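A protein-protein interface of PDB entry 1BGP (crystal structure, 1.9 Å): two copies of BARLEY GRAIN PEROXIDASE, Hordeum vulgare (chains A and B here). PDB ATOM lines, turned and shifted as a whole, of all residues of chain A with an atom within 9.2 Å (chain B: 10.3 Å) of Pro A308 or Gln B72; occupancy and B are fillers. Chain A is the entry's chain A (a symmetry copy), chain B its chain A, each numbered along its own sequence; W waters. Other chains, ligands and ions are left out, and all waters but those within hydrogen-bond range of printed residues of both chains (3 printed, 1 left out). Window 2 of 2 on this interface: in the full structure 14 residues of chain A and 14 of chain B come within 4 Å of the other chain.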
ATOM      1  N   ARG A 136      14.155 -22.493  11.734  1.00  0.00           N
ATOM      2  CA  ARG A 136      13.552 -22.341  13.051  1.00  0.00           C
ATOM      3  C   ARG A 136      12.042 -22.475  12.890  1.00  0.00           C
ATOM      4  O   ARG A 136      11.276 -22.175  13.811  1.00  0.00           O
ATOM      5  CB  ARG A 136      13.885 -20.976  13.660  1.00  0.00           C
ATOM      6  CG  ARG A 136      15.309 -20.834  14.151  1.00  0.00           C
ATOM      7  CD  ARG A 136      15.467 -19.584  15.013  1.00  0.00           C
ATOM      8  NE  ARG A 136      14.623 -19.642  16.208  1.00  0.00           N
ATOM      9  CZ  ARG A 136      15.025 -20.092  17.395  1.00  0.00           C
ATOM     10  NH1 ARG A 136      16.264 -20.525  17.562  1.00  0.00           N
ATOM     11  NH2 ARG A 136      14.180 -20.120  18.417  1.00  0.00           N
ATOM     12  N   SER A 137      11.619 -22.897  11.702  1.00  0.00           N
ATOM     13  CA  SER A 137      10.204 -23.073  11.403  1.00  0.00           C
ATOM     14  C   SER A 137       9.851 -24.553  11.382  1.00  0.00           C
ATOM     15  O   SER A 137      10.515 -25.346  10.709  1.00  0.00           O
ATOM     16  CB  SER A 137       9.869 -22.459  10.041  1.00  0.00           C
ATOM     17  OG  SER A 137      10.307 -21.114   9.956  1.00  0.00           O
ATOM     18  N   GLY A 295      18.980 -18.676   8.802  1.00  0.00           N
ATOM     19  CA  GLY A 295      18.764 -19.763   9.737  1.00  0.00           C
ATOM     20  C   GLY A 295      19.797 -19.766  10.833  1.00  0.00           C
ATOM     21  O   GLY A 295      20.393 -18.733  11.130  1.00  0.00           O
ATOM     22  N   GLU A 296      20.030 -20.931  11.420  1.00  0.00           N
ATOM     23  CA  GLU A 296      21.003 -21.051  12.490  1.00  0.00           C
ATOM     24  C   GLU A 296      21.716 -22.387  12.411  1.00  0.00           C
ATOM     25  O   GLU A 296      21.437 -23.205  11.533  1.00  0.00           O
ATOM     26  CB  GLU A 296      20.305 -20.923  13.849  1.00  0.00           C
ATOM     27  CG  GLU A 296      19.235 -21.989  14.096  1.00  0.00           C
ATOM     28  CD  GLU A 296      18.536 -21.842  15.438  1.00  0.00           C
ATOM     29  OE1 GLU A 296      18.527 -20.726  16.000  1.00  0.00           O
ATOM     30  OE2 GLU A 296      17.988 -22.848  15.930  1.00  0.00           O
ATOM     31  N   ARG A 299      22.486 -26.657  18.020  1.00  0.00           N
ATOM     32  CA  ARG A 299      23.372 -27.292  18.985  1.00  0.00           C
ATOM     33  C   ARG A 299      22.803 -28.684  19.258  1.00  0.00           C
ATOM     34  O   ARG A 299      23.411 -29.497  19.954  1.00  0.00           O
ATOM     35  CB  ARG A 299      23.428 -26.478  20.281  1.00  0.00           C
ATOM     36  CG  ARG A 299      23.762 -25.012  20.079  1.00  0.00           C
ATOM     37  CD  ARG A 299      23.691 -24.260  21.394  1.00  0.00           C
ATOM     38  NE  ARG A 299      23.471 -22.830  21.192  1.00  0.00           N
ATOM     39  CZ  ARG A 299      22.617 -22.094  21.902  1.00  0.00           C
ATOM     40  NH1 ARG A 299      21.895 -22.646  22.873  1.00  0.00           N
ATOM     41  NH2 ARG A 299      22.466 -20.805  21.627  1.00  0.00           N
ATOM     42  N   ARG A 304      15.195 -26.139  18.241  1.00  0.00           N
ATOM     43  CA  ARG A 304      15.706 -24.854  17.818  1.00  0.00           C
ATOM     44  C   ARG A 304      16.553 -24.369  18.986  1.00  0.00           C
ATOM     45  O   ARG A 304      16.319 -24.759  20.137  1.00  0.00           O
ATOM     46  CB  ARG A 304      14.547 -23.897  17.565  1.00  0.00           C
ATOM     47  CG  ARG A 304      13.601 -24.398  16.495  1.00  0.00           C
ATOM     48  CD  ARG A 304      12.365 -23.550  16.406  1.00  0.00           C
ATOM     49  NE  ARG A 304      11.544 -23.647  17.607  1.00  0.00           N
ATOM     50  CZ  ARG A 304      10.537 -22.827  17.882  1.00  0.00           C
ATOM     51  NH1 ARG A 304      10.228 -21.852  17.038  1.00  0.00           N
ATOM     52  NH2 ARG A 304       9.835 -22.986  18.995  1.00  0.00           N
ATOM     53  N   ASN A 305      17.578 -23.583  18.692  1.00  0.00           N
ATOM     54  CA  ASN A 305      18.440 -23.059  19.738  1.00  0.00           C
ATOM     55  C   ASN A 305      17.583 -22.206  20.662  1.00  0.00           C
ATOM     56  O   ASN A 305      16.886 -21.296  20.212  1.00  0.00           O
ATOM     57  CB  ASN A 305      19.584 -22.236  19.134  1.00  0.00           C
ATOM     58  CG  ASN A 305      20.587 -23.095  18.387  1.00  0.00           C
ATOM     59  OD1 ASN A 305      20.633 -24.316  18.565  1.00  0.00           O
ATOM     60  ND2 ASN A 305      21.402 -22.465  17.554  1.00  0.00           N
ATOM     61  N   PRO A 306      17.556 -22.548  21.959  1.00  0.00           N
ATOM     62  CA  PRO A 306      16.755 -21.787  22.918  1.00  0.00           C
ATOM     63  C   PRO A 306      17.279 -20.366  23.087  1.00  0.00           C
ATOM     64  O   PRO A 306      18.441 -20.083  22.790  1.00  0.00           O
ATOM     65  CB  PRO A 306      16.899 -22.606  24.198  1.00  0.00           C
ATOM     66  CG  PRO A 306      18.268 -23.185  24.073  1.00  0.00           C
ATOM     67  CD  PRO A 306      18.295 -23.631  22.630  1.00  0.00           C
ATOM     68  N   GLY A 307      16.417 -19.477  23.561  1.00  0.00           N
ATOM     69  CA  GLY A 307      16.822 -18.101  23.762  1.00  0.00           C
ATOM     70  C   GLY A 307      15.937 -17.128  23.013  1.00  0.00           C
ATOM     71  O   GLY A 307      15.317 -17.493  22.011  1.00  0.00           O
ATOM     72  N   PRO A 308      15.861 -15.871  23.481  1.00  0.00           N
ATOM     73  CA  PRO A 308      15.055 -14.798  22.888  1.00  0.00           C
ATOM     74  C   PRO A 308      15.579 -14.298  21.537  1.00  0.00           C
ATOM     75  O   PRO A 308      14.852 -13.643  20.785  1.00  0.00           O
ATOM     76  CB  PRO A 308      15.128 -13.703  23.951  1.00  0.00           C
ATOM     77  CG  PRO A 308      16.501 -13.896  24.525  1.00  0.00           C
ATOM     78  CD  PRO A 308      16.558 -15.395  24.690  1.00  0.00           C
ATOM     79  N   GLY A 309      16.841 -14.601  21.246  1.00  0.00           N
ATOM     80  CA  GLY A 309      17.448 -14.178  19.998  1.00  0.00           C
ATOM     81  C   GLY A 309      18.852 -14.739  19.872  1.00  0.00           C
ATOM     82  O   GLY A 309      19.612 -14.259  19.006  1.00  0.00           O
ATOM     83  OXT GLY A 309      19.195 -15.666  20.641  1.00  0.00           O
ATOM     84  N   ASP B  63       9.946 -27.668  23.025  1.00  0.00           N
ATOM     85  CA  ASP B  63      10.325 -26.689  22.014  1.00  0.00           C
ATOM     86  C   ASP B  63       9.173 -26.481  21.028  1.00  0.00           C
ATOM     87  O   ASP B  63       8.956 -25.377  20.535  1.00  0.00           O
ATOM     88  CB  ASP B  63      11.590 -27.156  21.280  1.00  0.00           C
ATOM     89  CG  ASP B  63      12.024 -26.199  20.179  1.00  0.00           C
ATOM     90  OD1 ASP B  63      12.120 -24.980  20.438  1.00  0.00           O
ATOM     91  OD2 ASP B  63      12.274 -26.671  19.052  1.00  0.00           O
ATOM     92  N   SER B  65       6.113 -26.325  21.666  1.00  0.00           N
ATOM     93  CA  SER B  65       4.996 -25.601  22.265  1.00  0.00           C
ATOM     94  C   SER B  65       5.112 -24.083  22.228  1.00  0.00           C
ATOM     95  O   SER B  65       6.215 -23.523  22.293  1.00  0.00           O
ATOM     96  CB  SER B  65       4.792 -26.047  23.716  1.00  0.00           C
ATOM     97  OG  SER B  65       4.344 -27.388  23.770  1.00  0.00           O
ATOM     98  N   ALA B  66       3.960 -23.425  22.118  1.00  0.00           N
ATOM     99  CA  ALA B  66       3.901 -21.970  22.119  1.00  0.00           C
ATOM    100  C   ALA B  66       4.425 -21.566  23.496  1.00  0.00           C
ATOM    101  O   ALA B  66       4.206 -22.281  24.471  1.00  0.00           O
ATOM    102  CB  ALA B  66       2.464 -21.497  21.930  1.00  0.00           C
ATOM    103  N   THR B  67       5.126 -20.439  23.561  1.00  0.00           N
ATOM    104  CA  THR B  67       5.738 -19.920  24.790  1.00  0.00           C
ATOM    105  C   THR B  67       6.812 -20.848  25.361  1.00  0.00           C
ATOM    106  O   THR B  67       7.320 -20.633  26.466  1.00  0.00           O
ATOM    107  CB  THR B  67       4.701 -19.512  25.886  1.00  0.00           C
ATOM    108  OG1 THR B  67       4.063 -20.671  26.442  1.00  0.00           O
ATOM    109  CG2 THR B  67       3.645 -18.583  25.308  1.00  0.00           C
ATOM    110  N   GLY B  68       7.189 -21.852  24.572  1.00  0.00           N
ATOM    111  CA  GLY B  68       8.217 -22.789  24.981  1.00  0.00           C
ATOM    112  C   GLY B  68       9.601 -22.168  24.907  1.00  0.00           C
ATOM    113  O   GLY B  68       9.731 -20.980  24.592  1.00  0.00           O
ATOM    114  N   PRO B  69      10.662 -22.959  25.133  1.00  0.00           N
ATOM    115  CA  PRO B  69      12.066 -22.543  25.113  1.00  0.00           C
ATOM    116  C   PRO B  69      12.596 -21.909  23.828  1.00  0.00           C
ATOM    117  O   PRO B  69      13.522 -21.099  23.883  1.00  0.00           O
ATOM    118  CB  PRO B  69      12.807 -23.835  25.456  1.00  0.00           C
ATOM    119  CG  PRO B  69      11.903 -24.894  24.920  1.00  0.00           C
ATOM    120  CD  PRO B  69      10.560 -24.408  25.374  1.00  0.00           C
ATOM    121  N   GLY B  70      12.019 -22.270  22.687  1.00  0.00           N
ATOM    122  CA  GLY B  70      12.474 -21.710  21.426  1.00  0.00           C
ATOM    123  C   GLY B  70      11.639 -20.536  20.954  1.00  0.00           C
ATOM    124  O   GLY B  70      11.844 -20.027  19.856  1.00  0.00           O
ATOM    125  N   GLU B  71      10.696 -20.099  21.781  1.00  0.00           N
ATOM    126  CA  GLU B  71       9.821 -18.986  21.433  1.00  0.00           C
ATOM    127  C   GLU B  71      10.571 -17.654  21.410  1.00  0.00           C
ATOM    128  O   GLU B  71      11.187 -17.264  22.402  1.00  0.00           O
ATOM    129  CB  GLU B  71       8.661 -18.910  22.428  1.00  0.00           C
ATOM    130  CG  GLU B  71       7.607 -17.871  22.100  1.00  0.00           C
ATOM    131  CD  GLU B  71       6.807 -18.218  20.861  1.00  0.00           C
ATOM    132  OE1 GLU B  71       5.980 -19.154  20.925  1.00  0.00           O
ATOM    133  OE2 GLU B  71       7.004 -17.554  19.823  1.00  0.00           O
ATOM    134  N   GLN B  72      10.517 -16.966  20.274  1.00  0.00           N
ATOM    135  CA  GLN B  72      11.180 -15.672  20.123  1.00  0.00           C
ATOM    136  C   GLN B  72      10.225 -14.607  19.589  1.00  0.00           C
ATOM    137  O   GLN B  72      10.571 -13.431  19.528  1.00  0.00           O
ATOM    138  CB  GLN B  72      12.362 -15.785  19.159  1.00  0.00           C
ATOM    139  CG  GLN B  72      13.447 -16.744  19.591  1.00  0.00           C
ATOM    140  CD  GLN B  72      14.579 -16.820  18.586  1.00  0.00           C
ATOM    141  OE1 GLN B  72      14.385 -16.568  17.394  1.00  0.00           O
ATOM    142  NE2 GLN B  72      15.767 -17.179  19.056  1.00  0.00           N
ATOM    143  N   GLN B  73       9.023 -15.024  19.204  1.00  0.00           N
ATOM    144  CA  GLN B  73       8.036 -14.107  18.642  1.00  0.00           C
ATOM    145  C   GLN B  73       7.068 -13.503  19.661  1.00  0.00           C
ATOM    146  O   GLN B  73       6.515 -12.426  19.436  1.00  0.00           O
ATOM    147  CB  GLN B  73       7.229 -14.809  17.539  1.00  0.00           C
ATOM    148  CG  GLN B  73       8.065 -15.577  16.512  1.00  0.00           C
ATOM    149  CD  GLN B  73       8.499 -16.950  17.011  1.00  0.00           C
ATOM    150  OE1 GLN B  73       9.597 -17.114  17.552  1.00  0.00           O
ATOM    151  NE2 GLN B  73       7.626 -17.937  16.856  1.00  0.00           N
ATOM    152  N   ALA B  74       6.854 -14.204  20.769  1.00  0.00           N
ATOM    153  CA  ALA B  74       5.929 -13.750  21.803  1.00  0.00           C
ATOM    154  C   ALA B  74       6.352 -12.461  22.500  1.00  0.00           C
ATOM    155  O   ALA B  74       7.542 -12.160  22.610  1.00  0.00           O
ATOM    156  CB  ALA B  74       5.714 -14.857  22.831  1.00  0.00           C
ATOM    157  N   PRO B  75       5.368 -11.662  22.954  1.00  0.00           N
ATOM    158  CA  PRO B  75       5.667 -10.407  23.645  1.00  0.00           C
ATOM    159  C   PRO B  75       6.313 -10.726  24.994  1.00  0.00           C
ATOM    160  O   PRO B  75       6.119 -11.819  25.536  1.00  0.00           O
ATOM    161  CB  PRO B  75       4.283  -9.773  23.807  1.00  0.00           C
ATOM    162  CG  PRO B  75       3.378 -10.957  23.909  1.00  0.00           C
ATOM    163  CD  PRO B  75       3.912 -11.852  22.825  1.00  0.00           C
ATOM    164  N   PRO B  76       7.059  -9.766  25.569  1.00  0.00           N
ATOM    165  CA  PRO B  76       7.751  -9.916  26.855  1.00  0.00           C
ATOM    166  C   PRO B  76       6.951 -10.612  27.954  1.00  0.00           C
ATOM    167  O   PRO B  76       7.478 -11.469  28.664  1.00  0.00           O
ATOM    168  CB  PRO B  76       8.070  -8.473  27.228  1.00  0.00           C
ATOM    169  CG  PRO B  76       8.370  -7.862  25.898  1.00  0.00           C
ATOM    170  CD  PRO B  76       7.243  -8.401  25.038  1.00  0.00           C
ATOM    171  N   LEU B  78       4.899 -12.887  27.743  1.00  0.00           N
ATOM    172  CA  LEU B  78       4.603 -14.275  27.410  1.00  0.00           C
ATOM    173  C   LEU B  78       5.872 -15.088  27.188  1.00  0.00           C
ATOM    174  O   LEU B  78       5.809 -16.258  26.812  1.00  0.00           O
ATOM    175  CB  LEU B  78       3.716 -14.330  26.167  1.00  0.00           C
ATOM    176  CG  LEU B  78       2.333 -14.961  26.346  1.00  0.00           C
ATOM    177  CD1 LEU B  78       1.656 -14.434  27.599  1.00  0.00           C
ATOM    178  CD2 LEU B  78       1.486 -14.687  25.118  1.00  0.00           C
ATOM    179  N   THR B  79       7.015 -14.467  27.443  1.00  0.00           N
ATOM    180  CA  THR B  79       8.304 -15.116  27.280  1.00  0.00           C
ATOM    181  C   THR B  79       8.851 -15.458  28.661  1.00  0.00           C
ATOM    182  O   THR B  79       9.060 -14.569  29.483  1.00  0.00           O
ATOM    183  CB  THR B  79       9.288 -14.175  26.570  1.00  0.00           C
ATOM    184  OG1 THR B  79       8.675 -13.669  25.378  1.00  0.00           O
ATOM    185  CG2 THR B  79      10.567 -14.911  26.205  1.00  0.00           C
ATOM    186  N   LEU B  80       9.059 -16.744  28.921  1.00  0.00           N
ATOM    187  CA  LEU B  80       9.579 -17.193  30.208  1.00  0.00           C
ATOM    188  C   LEU B  80      11.103 -17.051  30.256  1.00  0.00           C
ATOM    189  O   LEU B  80      11.752 -16.922  29.211  1.00  0.00           O
ATOM    190  CB  LEU B  80       9.177 -18.650  30.459  1.00  0.00           C
ATOM    191  CG  LEU B  80       7.708 -19.002  30.736  1.00  0.00           C
ATOM    192  CD1 LEU B  80       7.271 -18.424  32.061  1.00  0.00           C
ATOM    193  CD2 LEU B  80       6.806 -18.517  29.619  1.00  0.00           C
ATOM    194  N   ARG B  81      11.670 -17.068  31.460  1.00  0.00           N
ATOM    195  CA  ARG B  81      13.119 -16.944  31.630  1.00  0.00           C
ATOM    196  C   ARG B  81      13.871 -18.102  31.002  1.00  0.00           C
ATOM    197  O   ARG B  81      13.611 -19.265  31.318  1.00  0.00           O
ATOM    198  CB  ARG B  81      13.507 -16.890  33.109  1.00  0.00           C
ATOM    199  CG  ARG B  81      13.117 -15.622  33.833  1.00  0.00           C
ATOM    200  CD  ARG B  81      13.878 -15.514  35.141  1.00  0.00           C
ATOM    201  NE  ARG B  81      13.347 -14.449  35.987  1.00  0.00           N
ATOM    202  CZ  ARG B  81      14.076 -13.486  36.536  1.00  0.00           C
ATOM    203  NH1 ARG B  81      15.386 -13.442  36.339  1.00  0.00           N
ATOM    204  NH2 ARG B  81      13.488 -12.548  37.269  1.00  0.00           N
ATOM    205  N   PRO B  82      14.836 -17.805  30.121  1.00  0.00           N
ATOM    206  CA  PRO B  82      15.611 -18.871  29.481  1.00  0.00           C
ATOM    207  C   PRO B  82      16.305 -19.737  30.534  1.00  0.00           C
ATOM    208  O   PRO B  82      16.378 -20.963  30.399  1.00  0.00           O
ATOM    209  CB  PRO B  82      16.624 -18.091  28.643  1.00  0.00           C
ATOM    210  CG  PRO B  82      15.856 -16.867  28.256  1.00  0.00           C
ATOM    211  CD  PRO B  82      15.177 -16.490  29.553  1.00  0.00           C
ATOM    212  N   SER B  83      16.775 -19.098  31.603  1.00  0.00           N
ATOM    213  CA  SER B  83      17.459 -19.799  32.684  1.00  0.00           C
ATOM    214  C   SER B  83      16.549 -20.787  33.414  1.00  0.00           C
ATOM    215  O   SER B  83      17.035 -21.750  34.012  1.00  0.00           O
ATOM    216  CB  SER B  83      18.031 -18.796  33.683  1.00  0.00           C
ATOM    217  OG  SER B  83      17.002 -17.984  34.218  1.00  0.00           O
ATOM    218  N   ALA B  84      15.243 -20.532  33.394  1.00  0.00           N
ATOM    219  CA  ALA B  84      14.279 -21.415  34.046  1.00  0.00           C
ATOM    220  C   ALA B  84      14.185 -22.730  33.270  1.00  0.00           C
ATOM    221  O   ALA B  84      14.222 -23.810  33.861  1.00  0.00           O
ATOM    222  CB  ALA B  84      12.909 -20.746  34.132  1.00  0.00           C
ATOM    223  N   PHE B  85      14.085 -22.634  31.944  1.00  0.00           N
ATOM    224  CA  PHE B  85      14.010 -23.826  31.092  1.00  0.00           C
ATOM    225  C   PHE B  85      15.290 -24.636  31.268  1.00  0.00           C
ATOM    226  O   PHE B  85      15.257 -25.860  31.433  1.00  0.00           O
ATOM    227  CB  PHE B  85      13.862 -23.440  29.616  1.00  0.00           C
ATOM    228  CG  PHE B  85      12.522 -22.852  29.263  1.00  0.00           C
ATOM    229  CD1 PHE B  85      11.370 -23.632  29.308  1.00  0.00           C
ATOM    230  CD2 PHE B  85      12.419 -21.529  28.846  1.00  0.00           C
ATOM    231  CE1 PHE B  85      10.134 -23.103  28.941  1.00  0.00           C
ATOM    232  CE2 PHE B  85      11.188 -20.988  28.476  1.00  0.00           C
ATOM    233  CZ  PHE B  85      10.043 -21.778  28.523  1.00  0.00           C
ATOM    234  N   ASP B 219      10.805  -0.487  27.029  1.00  0.00           N
ATOM    235  CA  ASP B 219      11.464  -1.760  27.262  1.00  0.00           C
ATOM    236  C   ASP B 219      12.233  -1.672  28.573  1.00  0.00           C
ATOM    237  O   ASP B 219      13.407  -1.285  28.607  1.00  0.00           O
ATOM    238  CB  ASP B 219      12.409  -2.113  26.113  1.00  0.00           C
ATOM    239  CG  ASP B 219      13.129  -3.436  26.338  1.00  0.00           C
ATOM    240  OD1 ASP B 219      12.478  -4.405  26.786  1.00  0.00           O
ATOM    241  OD2 ASP B 219      14.348  -3.503  26.083  1.00  0.00           O
ATOM    242  N   ARG B 221      11.868  -3.332  32.974  1.00  0.00           N
ATOM    243  CA  ARG B 221      11.160  -4.174  33.925  1.00  0.00           C
ATOM    244  C   ARG B 221      11.229  -3.546  35.301  1.00  0.00           C
ATOM    245  O   ARG B 221      12.075  -2.687  35.561  1.00  0.00           O
ATOM    246  CB  ARG B 221      11.795  -5.560  33.980  1.00  0.00           C
ATOM    247  CG  ARG B 221      11.822  -6.275  32.646  1.00  0.00           C
ATOM    248  CD  ARG B 221      12.661  -7.532  32.708  1.00  0.00           C
ATOM    249  NE  ARG B 221      12.840  -8.108  31.379  1.00  0.00           N
ATOM    250  CZ  ARG B 221      11.937  -8.861  30.759  1.00  0.00           C
ATOM    251  NH1 ARG B 221      10.777  -9.144  31.346  1.00  0.00           N
ATOM    252  NH2 ARG B 221      12.187  -9.317  29.538  1.00  0.00           N
HETATM  253  O   HOH W   1      14.559 -20.095  26.193  1.00  0.00           O
HETATM  254  O   HOH W   2       7.429 -21.080  16.808  1.00  0.00           O
HETATM  255  O   HOH W   3      14.437 -24.802  22.171  1.00  0.00           O
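The guanidinium group (NE) of Arg A304 lies within salt-bridge range of the side-chain carboxylate (OD1) of Asp B63 (3.2 Å).
O of Pro B69 lies within hydrogen-bond range of N of Gly A307 (3.3 Å).
NH2 of Arg A136 lies within hydrogen-bond range of O of Gly B70, 2.7 Å away.
The guanidinium group of Arg A136 sits at hydrogen-bond distance from the side-chain amide oxygen of Gln B72 (3.3 Å).
NE2 of Gln B72 lies within hydrogen-bond range of O of Gly A307, at 3.0 Å.
NH1 of Arg A136 lies within salt-bridge range of OE1 of Glu A296 (2.8 Å).
The backbone carbonyl oxygen (O) of Arg A136 lies close to the guanidinium group (NH1) of Arg A304.
O of Asn A305 is in hydrogen-bond range of NH1 of Arg A136, at 2.8 Å.
Gly B70 touches Arg A304 (C to NH2, 3.6 Å).
Pro B69 touches Pro A306 (O to CA, 3.4 Å).
Pro A308 touches Gln B72 (O to CG, 3.6 Å).
CD of Pro A308 touches CG of Pro B82, 3.9 Å away.
N of Gly A309 touches NE2 of Gln B72, at 3.5 Å.
Printed residues of chain B within 4 Å of Arg A136: Gly B70 (2.7 Å) and Gln B72 (3.3 Å).
Arg A299 touches none of the printed residues of chain B.
Pro A308 touches just these residues of chain B: Gln B72 (3.6 Å) and Pro B82 (3.9 Å).
Of the printed residues of chain A, Gly B70 touches Arg A136 and Arg A304.
Gln B72 touches just these residues of chain A: Arg A136 (3.3 Å), Gly A307 (3.0 Å), Pro A308 (3.6 Å) and Gly A309 (3.5 Å).
Leu B78 touches none of the printed residues of chain A.
The nearest residue of chain B that does not touch Pro A308 is Glu B71 (4.6 Å).
Of the 23 printed residues of chain B, 5 touch a printed residue of chain A.
Hydrophobic or aromatic side chains of chain B that line the printed part of chain A: Pro B82.
Hydrophobic or aromatic side chains of chain A that line the printed part of chain B: Pro A306 and Pro A308.
Among the printed residues, 10 pairs touch across the chains.
Among the printed residues, Asp or Glu carboxylates within 4 Å of a Lys or Arg side-chain nitrogen of the other chain: Arg A304 with Asp B63.
No position is printed for both chains.
Of the 10 pairs that touch across the chains among the printed residues, none has its exchanged pair printed and touching as well.
Water W1 lies within hydrogen-bond range of O of Pro B69 (2.7 Å) and N of Gly A307 (3.3 Å).
Water W3 lies within hydrogen-bond range of O of Arg A304 (2.8 Å) and OD1 of Asp B63 (2.9 Å).
Water W2 lies within hydrogen-bond range of NH1 of Arg A304 (2.9 Å) and NE2 of Gln B73 (3.1 Å).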
